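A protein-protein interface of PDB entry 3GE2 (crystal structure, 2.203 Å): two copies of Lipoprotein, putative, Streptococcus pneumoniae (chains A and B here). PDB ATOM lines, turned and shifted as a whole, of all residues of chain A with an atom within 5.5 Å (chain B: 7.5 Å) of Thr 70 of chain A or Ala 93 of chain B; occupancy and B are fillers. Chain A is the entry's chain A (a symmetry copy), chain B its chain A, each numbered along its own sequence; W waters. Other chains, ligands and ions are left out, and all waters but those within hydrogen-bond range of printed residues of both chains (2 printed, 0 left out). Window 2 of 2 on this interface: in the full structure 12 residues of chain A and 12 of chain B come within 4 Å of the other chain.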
ATOM      1  N   THR A  68      15.500   0.396  15.822  1.00  0.00           N
ATOM      2  CA  THR A  68      16.797  -0.261  15.822  1.00  0.00           C
ATOM      3  C   THR A  68      16.607  -1.649  15.213  1.00  0.00           C
ATOM      4  O   THR A  68      15.935  -2.472  15.828  1.00  0.00           O
ATOM      5  CB  THR A  68      17.297  -0.484  17.300  1.00  0.00           C
ATOM      6  OG1 THR A  68      16.338  -1.289  18.023  1.00  0.00           O
ATOM      7  CG2 THR A  68      17.430   0.847  18.034  1.00  0.00           C
ATOM      8  N   GLY A  69      17.189  -1.922  14.040  1.00  0.00           N
ATOM      9  CA  GLY A  69      17.060  -3.233  13.407  1.00  0.00           C
ATOM     10  C   GLY A  69      15.581  -3.478  13.021  1.00  0.00           C
ATOM     11  O   GLY A  69      14.970  -2.726  12.253  1.00  0.00           O
ATOM     12  N   THR A  70      14.955  -4.479  13.620  1.00  0.00           N
ATOM     13  CA  THR A  70      13.590  -4.777  13.241  1.00  0.00           C
ATOM     14  C   THR A  70      12.645  -4.496  14.383  1.00  0.00           C
ATOM     15  O   THR A  70      11.499  -4.973  14.370  1.00  0.00           O
ATOM     16  CB  THR A  70      13.419  -6.259  12.863  1.00  0.00           C
ATOM     17  OG1 THR A  70      13.740  -7.046  14.001  1.00  0.00           O
ATOM     18  CG2 THR A  70      14.371  -6.658  11.732  1.00  0.00           C
ATOM     19  N   THR A  71      13.122  -3.760  15.380  1.00  0.00           N
ATOM     20  CA  THR A  71      12.248  -3.392  16.491  1.00  0.00           C
ATOM     21  C   THR A  71      12.355  -1.908  16.781  1.00  0.00           C
ATOM     22  O   THR A  71      13.185  -1.235  16.207  1.00  0.00           O
ATOM     23  CB  THR A  71      12.629  -4.161  17.793  1.00  0.00           C
ATOM     24  OG1 THR A  71      13.978  -3.843  18.157  1.00  0.00           O
ATOM     25  CG2 THR A  71      12.554  -5.677  17.601  1.00  0.00           C
ATOM     26  N   GLY A  72      11.591  -1.426  17.759  1.00  0.00           N
ATOM     27  CA  GLY A  72      11.681  -0.049  18.175  1.00  0.00           C
ATOM     28  C   GLY A  72      10.756   0.291  19.314  1.00  0.00           C
ATOM     29  O   GLY A  72      10.107  -0.598  19.858  1.00  0.00           O
ATOM     30  N   VAL A  88       7.560  -1.748  19.609  1.00  0.00           N
ATOM     31  CA  VAL A  88       7.250  -1.813  18.179  1.00  0.00           C
ATOM     32  C   VAL A  88       8.027  -2.919  17.526  1.00  0.00           C
ATOM     33  O   VAL A  88       9.176  -3.132  17.877  1.00  0.00           O
ATOM     34  CB  VAL A  88       7.735  -0.598  17.458  1.00  0.00           C
ATOM     35  CG1 VAL A  88       6.802  -0.249  16.445  1.00  0.00           C
ATOM     36  CG2 VAL A  88       7.795   0.540  18.399  1.00  0.00           C
ATOM     37  N   THR A  89       7.422  -3.580  16.542  1.00  0.00           N
ATOM     38  CA  THR A  89       8.165  -4.540  15.741  1.00  0.00           C
ATOM     39  C   THR A  89       7.775  -4.257  14.319  1.00  0.00           C
ATOM     40  O   THR A  89       6.587  -3.940  14.026  1.00  0.00           O
ATOM     41  CB  THR A  89       7.844  -6.031  16.022  1.00  0.00           C
ATOM     42  OG1 THR A  89       6.430  -6.209  15.981  1.00  0.00           O
ATOM     43  CG2 THR A  89       8.333  -6.453  17.425  1.00  0.00           C
ATOM     44  N   PHE A  90       8.782  -4.400  13.455  1.00  0.00           N
ATOM     45  CA  PHE A  90       8.666  -4.158  12.031  1.00  0.00           C
ATOM     46  C   PHE A  90       8.815  -5.426  11.222  1.00  0.00           C
ATOM     47  O   PHE A  90       9.836  -6.135  11.292  1.00  0.00           O
ATOM     48  CB  PHE A  90       9.700  -3.137  11.581  1.00  0.00           C
ATOM     49  CG  PHE A  90       9.509  -1.796  12.210  1.00  0.00           C
ATOM     50  CD1 PHE A  90       8.831  -0.801  11.548  1.00  0.00           C
ATOM     51  CD2 PHE A  90      10.099  -1.513  13.448  1.00  0.00           C
ATOM     52  CE1 PHE A  90       8.648   0.459  12.165  1.00  0.00           C
ATOM     53  CE2 PHE A  90       9.981  -0.262  14.047  1.00  0.00           C
ATOM     54  CZ  PHE A  90       9.239   0.724  13.409  1.00  0.00           C
ATOM     55  N   ASP A  91       7.763  -5.722  10.479  1.00  0.00           N
ATOM     56  CA  ASP A  91       7.762  -6.849   9.555  1.00  0.00           C
ATOM     57  C   ASP A  91       7.937  -6.290   8.147  1.00  0.00           C
ATOM     58  O   ASP A  91       6.976  -5.919   7.501  1.00  0.00           O
ATOM     59  CB  ASP A  91       6.437  -7.616   9.686  1.00  0.00           C
ATOM     60  CG  ASP A  91       6.253  -8.738   8.629  1.00  0.00           C
ATOM     61  OD1 ASP A  91       6.983  -8.811   7.610  1.00  0.00           O
ATOM     62  OD2 ASP A  91       5.342  -9.575   8.857  1.00  0.00           O
ATOM     63  N   PRO B  43      12.687 -11.401  21.088  1.00  0.00           N
ATOM     64  CA  PRO B  43      12.169 -12.303  20.056  1.00  0.00           C
ATOM     65  C   PRO B  43      13.277 -13.164  19.461  1.00  0.00           C
ATOM     66  O   PRO B  43      14.324 -12.629  19.100  1.00  0.00           O
ATOM     67  CB  PRO B  43      11.688 -11.347  18.968  1.00  0.00           C
ATOM     68  CG  PRO B  43      12.321  -9.935  19.317  1.00  0.00           C
ATOM     69  CD  PRO B  43      13.213 -10.158  20.512  1.00  0.00           C
ATOM     70  N   VAL B  44      13.037 -14.465  19.327  1.00  0.00           N
ATOM     71  CA  VAL B  44      13.940 -15.335  18.592  1.00  0.00           C
ATOM     72  C   VAL B  44      13.502 -15.475  17.141  1.00  0.00           C
ATOM     73  O   VAL B  44      12.363 -15.862  16.862  1.00  0.00           O
ATOM     74  CB  VAL B  44      13.953 -16.752  19.241  1.00  0.00           C
ATOM     75  CG1 VAL B  44      14.855 -17.710  18.495  1.00  0.00           C
ATOM     76  CG2 VAL B  44      14.378 -16.633  20.689  1.00  0.00           C
ATOM     77  N   ALA B  45      14.433 -15.254  16.228  1.00  0.00           N
ATOM     78  CA  ALA B  45      14.125 -15.194  14.827  1.00  0.00           C
ATOM     79  C   ALA B  45      13.774 -16.596  14.328  1.00  0.00           C
ATOM     80  O   ALA B  45      14.348 -17.567  14.762  1.00  0.00           O
ATOM     81  CB  ALA B  45      15.318 -14.573  14.029  1.00  0.00           C
ATOM     82  N   GLN B  46      12.807 -16.701  13.434  1.00  0.00           N
ATOM     83  CA  GLN B  46      12.379 -18.020  12.951  1.00  0.00           C
ATOM     84  C   GLN B  46      12.902 -18.329  11.537  1.00  0.00           C
ATOM     85  O   GLN B  46      13.212 -17.422  10.790  1.00  0.00           O
ATOM     86  CB  GLN B  46      10.844 -18.069  12.975  1.00  0.00           C
ATOM     87  CG  GLN B  46      10.332 -17.872  14.372  1.00  0.00           C
ATOM     88  CD  GLN B  46      10.771 -19.034  15.263  1.00  0.00           C
ATOM     89  OE1 GLN B  46      10.566 -20.192  14.910  1.00  0.00           O
ATOM     90  NE2 GLN B  46      11.361 -18.726  16.430  1.00  0.00           N
ATOM     91  N   PRO B  47      12.962 -19.617  11.163  1.00  0.00           N
ATOM     92  CA  PRO B  47      13.247 -20.009   9.779  1.00  0.00           C
ATOM     93  C   PRO B  47      12.304 -19.278   8.844  1.00  0.00           C
ATOM     94  O   PRO B  47      11.133 -19.070   9.171  1.00  0.00           O
ATOM     95  CB  PRO B  47      12.878 -21.500   9.755  1.00  0.00           C
ATOM     96  CG  PRO B  47      12.898 -21.922  11.091  1.00  0.00           C
ATOM     97  CD  PRO B  47      12.598 -20.781  11.980  1.00  0.00           C
ATOM     98  N   THR B  48      12.792 -18.912   7.676  1.00  0.00           N
ATOM     99  CA  THR B  48      11.987 -18.098   6.772  1.00  0.00           C
ATOM    100  C   THR B  48      11.234 -18.977   5.780  1.00  0.00           C
ATOM    101  O   THR B  48      10.248 -18.557   5.200  1.00  0.00           O
ATOM    102  CB  THR B  48      12.881 -17.139   5.970  1.00  0.00           C
ATOM    103  OG1 THR B  48      13.901 -17.924   5.322  1.00  0.00           O
ATOM    104  CG2 THR B  48      13.549 -16.060   6.971  1.00  0.00           C
ATOM    105  N   PHE B  90       3.471 -13.532   8.520  1.00  0.00           N
ATOM    106  CA  PHE B  90       4.579 -14.015   9.320  1.00  0.00           C
ATOM    107  C   PHE B  90       5.756 -13.067   9.295  1.00  0.00           C
ATOM    108  O   PHE B  90       6.315 -12.740   8.232  1.00  0.00           O
ATOM    109  CB  PHE B  90       5.018 -15.391   8.845  1.00  0.00           C
ATOM    110  CG  PHE B  90       3.955 -16.430   9.003  1.00  0.00           C
ATOM    111  CD1 PHE B  90       3.942 -17.257  10.100  1.00  0.00           C
ATOM    112  CD2 PHE B  90       3.012 -16.627   7.987  1.00  0.00           C
ATOM    113  CE1 PHE B  90       2.920 -18.226  10.240  1.00  0.00           C
ATOM    114  CE2 PHE B  90       2.033 -17.613   8.078  1.00  0.00           C
ATOM    115  CZ  PHE B  90       1.979 -18.406   9.217  1.00  0.00           C
ATOM    116  N   ASP B  91       6.103 -12.600  10.481  1.00  0.00           N
ATOM    117  CA  ASP B  91       7.275 -11.757  10.669  1.00  0.00           C
ATOM    118  C   ASP B  91       8.373 -12.623  11.277  1.00  0.00           C
ATOM    119  O   ASP B  91       8.448 -12.779  12.481  1.00  0.00           O
ATOM    120  CB  ASP B  91       6.920 -10.584  11.594  1.00  0.00           C
ATOM    121  CG  ASP B  91       8.138  -9.712  12.001  1.00  0.00           C
ATOM    122  OD1 ASP B  91       9.318 -10.100  11.820  1.00  0.00           O
ATOM    123  OD2 ASP B  91       7.877  -8.591  12.511  1.00  0.00           O
ATOM    124  N   SER B  92       9.261 -13.143  10.443  1.00  0.00           N
ATOM    125  CA  SER B  92      10.201 -14.147  10.936  1.00  0.00           C
ATOM    126  C   SER B  92      11.228 -13.586  11.875  1.00  0.00           C
ATOM    127  O   SER B  92      11.574 -14.254  12.846  1.00  0.00           O
ATOM    128  CB  SER B  92      10.877 -14.945   9.808  1.00  0.00           C
ATOM    129  OG  SER B  92      11.532 -14.077   8.951  1.00  0.00           O
ATOM    130  N   ALA B  93      11.715 -12.376  11.605  1.00  0.00           N
ATOM    131  CA  ALA B  93      12.768 -11.797  12.469  1.00  0.00           C
ATOM    132  C   ALA B  93      12.241 -11.537  13.876  1.00  0.00           C
ATOM    133  O   ALA B  93      12.957 -11.661  14.816  1.00  0.00           O
ATOM    134  CB  ALA B  93      13.323 -10.460  11.887  1.00  0.00           C
ATOM    135  N   ASN B  94      10.991 -11.145  14.027  1.00  0.00           N
ATOM    136  CA  ASN B  94      10.515 -10.855  15.386  1.00  0.00           C
ATOM    137  C   ASN B  94       9.595 -11.955  15.908  1.00  0.00           C
ATOM    138  O   ASN B  94       8.906 -11.741  16.896  1.00  0.00           O
ATOM    139  CB  ASN B  94       9.734  -9.528  15.394  1.00  0.00           C
ATOM    140  CG  ASN B  94      10.566  -8.364  14.844  1.00  0.00           C
ATOM    141  OD1 ASN B  94      10.171  -7.654  13.888  1.00  0.00           O
ATOM    142  ND2 ASN B  94      11.724  -8.200  15.401  1.00  0.00           N
ATOM    143  N   GLN B  95       9.494 -13.064  15.174  1.00  0.00           N
ATOM    144  CA  GLN B  95       8.733 -14.210  15.664  1.00  0.00           C
ATOM    145  C   GLN B  95       7.252 -13.811  15.917  1.00  0.00           C
ATOM    146  O   GLN B  95       6.644 -14.267  16.879  1.00  0.00           O
ATOM    147  CB  GLN B  95       9.449 -14.664  16.958  1.00  0.00           C
ATOM    148  CG  GLN B  95       8.702 -15.488  17.860  1.00  0.00           C
ATOM    149  CD  GLN B  95       9.550 -16.174  18.898  1.00  0.00           C
ATOM    150  OE1 GLN B  95      10.288 -15.564  19.674  1.00  0.00           O
ATOM    151  NE2 GLN B  95       9.450 -17.449  18.899  1.00  0.00           N
ATOM    152  N   ARG B  96       6.679 -12.947  15.079  1.00  0.00           N
ATOM    153  CA  ARG B  96       5.266 -12.581  15.209  1.00  0.00           C
ATOM    154  C   ARG B  96       4.393 -13.050  14.051  1.00  0.00           C
ATOM    155  O   ARG B  96       4.694 -12.820  12.873  1.00  0.00           O
ATOM    156  CB  ARG B  96       5.082 -11.044  15.296  1.00  0.00           C
ATOM    157  CG  ARG B  96       5.880 -10.365  16.442  1.00  0.00           C
ATOM    158  CD  ARG B  96       5.261 -10.604  17.772  1.00  0.00           C
ATOM    159  NE  ARG B  96       5.800  -9.727  18.802  1.00  0.00           N
ATOM    160  CZ  ARG B  96       6.771 -10.086  19.659  1.00  0.00           C
ATOM    161  NH1 ARG B  96       7.339 -11.289  19.594  1.00  0.00           N
ATOM    162  NH2 ARG B  96       7.178  -9.246  20.594  1.00  0.00           N
ATOM    163  N   TYR B 106       4.908 -17.081  17.218  1.00  0.00           N
ATOM    164  CA  TYR B 106       4.993 -18.436  16.686  1.00  0.00           C
ATOM    165  C   TYR B 106       6.409 -18.981  16.781  1.00  0.00           C
ATOM    166  O   TYR B 106       7.382 -18.219  16.753  1.00  0.00           O
ATOM    167  CB  TYR B 106       4.522 -18.495  15.210  1.00  0.00           C
ATOM    168  CG  TYR B 106       5.463 -17.913  14.172  1.00  0.00           C
ATOM    169  CD1 TYR B 106       6.104 -18.727  13.239  1.00  0.00           C
ATOM    170  CD2 TYR B 106       5.645 -16.518  14.066  1.00  0.00           C
ATOM    171  CE1 TYR B 106       6.930 -18.171  12.213  1.00  0.00           C
ATOM    172  CE2 TYR B 106       6.462 -15.955  13.059  1.00  0.00           C
ATOM    173  CZ  TYR B 106       7.116 -16.805  12.149  1.00  0.00           C
ATOM    174  OH  TYR B 106       7.881 -16.252  11.171  1.00  0.00           O
HETATM  175  O   HOH W   1       5.037  -7.119  18.413  1.00  0.00           O
HETATM  176  O   HOH W   2       5.974  -6.974  13.358  1.00  0.00           O
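Of the 14 printed residues of chain B, 4 touch a printed residue of chain A.
Among the printed residues, no Asp or Glu carboxylate lies within 4 Å of a Lys or Arg side-chain nitrogen of the other chain.
The side-chain carboxylate (OD1) of Asp 91 of chain B sits at hydrogen-bond distance from the backbone NH (N) of Ala 93 of chain B, 3.3 Å away.
The side-chain carboxylate (OD2) of Asp 91 of chain B sits close to the side-chain amide oxygen (OD1) of Asn 94 of chain B (2.8 Å).
The backbone NH (N) of Asp 91 of chain B is in hydrogen-bond range of the backbone carbonyl oxygen (O) of Arg 96 of chain B, at 2.8 Å.
The backbone carbonyl oxygen of Asn 94 of chain B is in hydrogen-bond range of the guanidinium group of Arg 96 of chain B, 3.2 Å away.
The backbone carbonyl oxygen (O) of Thr 68 of chain A lies within hydrogen-bond range of the side-chain hydroxyl (OG1) of Thr 71 of chain A.
N of Phe 90 of chain A is in hydrogen-bond range of O of Thr 70 of chain A.
Phe 90 of chain A touches Asp 91 of chain B, and with the chains exchanged Asp 91 of chain A touches Phe 90 of chain B.
Asp 91 of chain A touches its own counterpart, Asp 91 of chain B.
Water W2 lies within hydrogen-bond range of OD2 of Asp 91 of chain B and OG1 of Thr 89 of chain A.
Water W1 bridges the guanidinium group of Arg 96 of chain B (2.7 Å) and the side-chain hydroxyl of Thr 89 of chain A (2.9 Å).
The side-chain hydroxyl of Thr 70 of chain A sits at hydrogen-bond distance from the side-chain amide nitrogen of Asn 94 of chain B.
OD1 of Asn 94 of chain B lies close to O of Phe 90 of chain A (3.0 Å).
O of Phe 90 of chain A sits close to OD2 of Asp 91 of chain B, at 3.4 Å.
The backbone carbonyl oxygen (O) of Phe 90 of chain B lies close to the side-chain carboxylate (OD2) of Asp 91 of chain A (3.4 Å).
Among the printed residues, pairs that only touch across the chains: Thr 70 of chain A with Ala 93 of chain B, Thr 71 of chain A with Asn 94 of chain B, Thr 89 of chain A with Asn 94 of chain B and Asp 91 of chain A with Asp 91 of chain B.
Thr 68 of chain A touches none of the printed residues of chain B.
Of the printed residues of chain B, Thr 71 of chain A touches Asn 94 (3.4 Å).
Of the printed residues of chain B, Thr 89 of chain A touches Asn 94 (3.6 Å).
Printed residues of chain B within 4 Å of Asp 91 of chain A: Phe 90 (3.4 Å) and Asp 91 (3.3 Å).
Ala 93 of chain B touches one residue of chain A.
Printed residues of chain A within 4 Å of Asn 94 of chain B: Thr 70, Thr 71, Thr 89 and Phe 90.
The nearest printed residue of chain A that does not touch Ala 93 of chain B is Phe 90 of chain A (5.6 Å).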
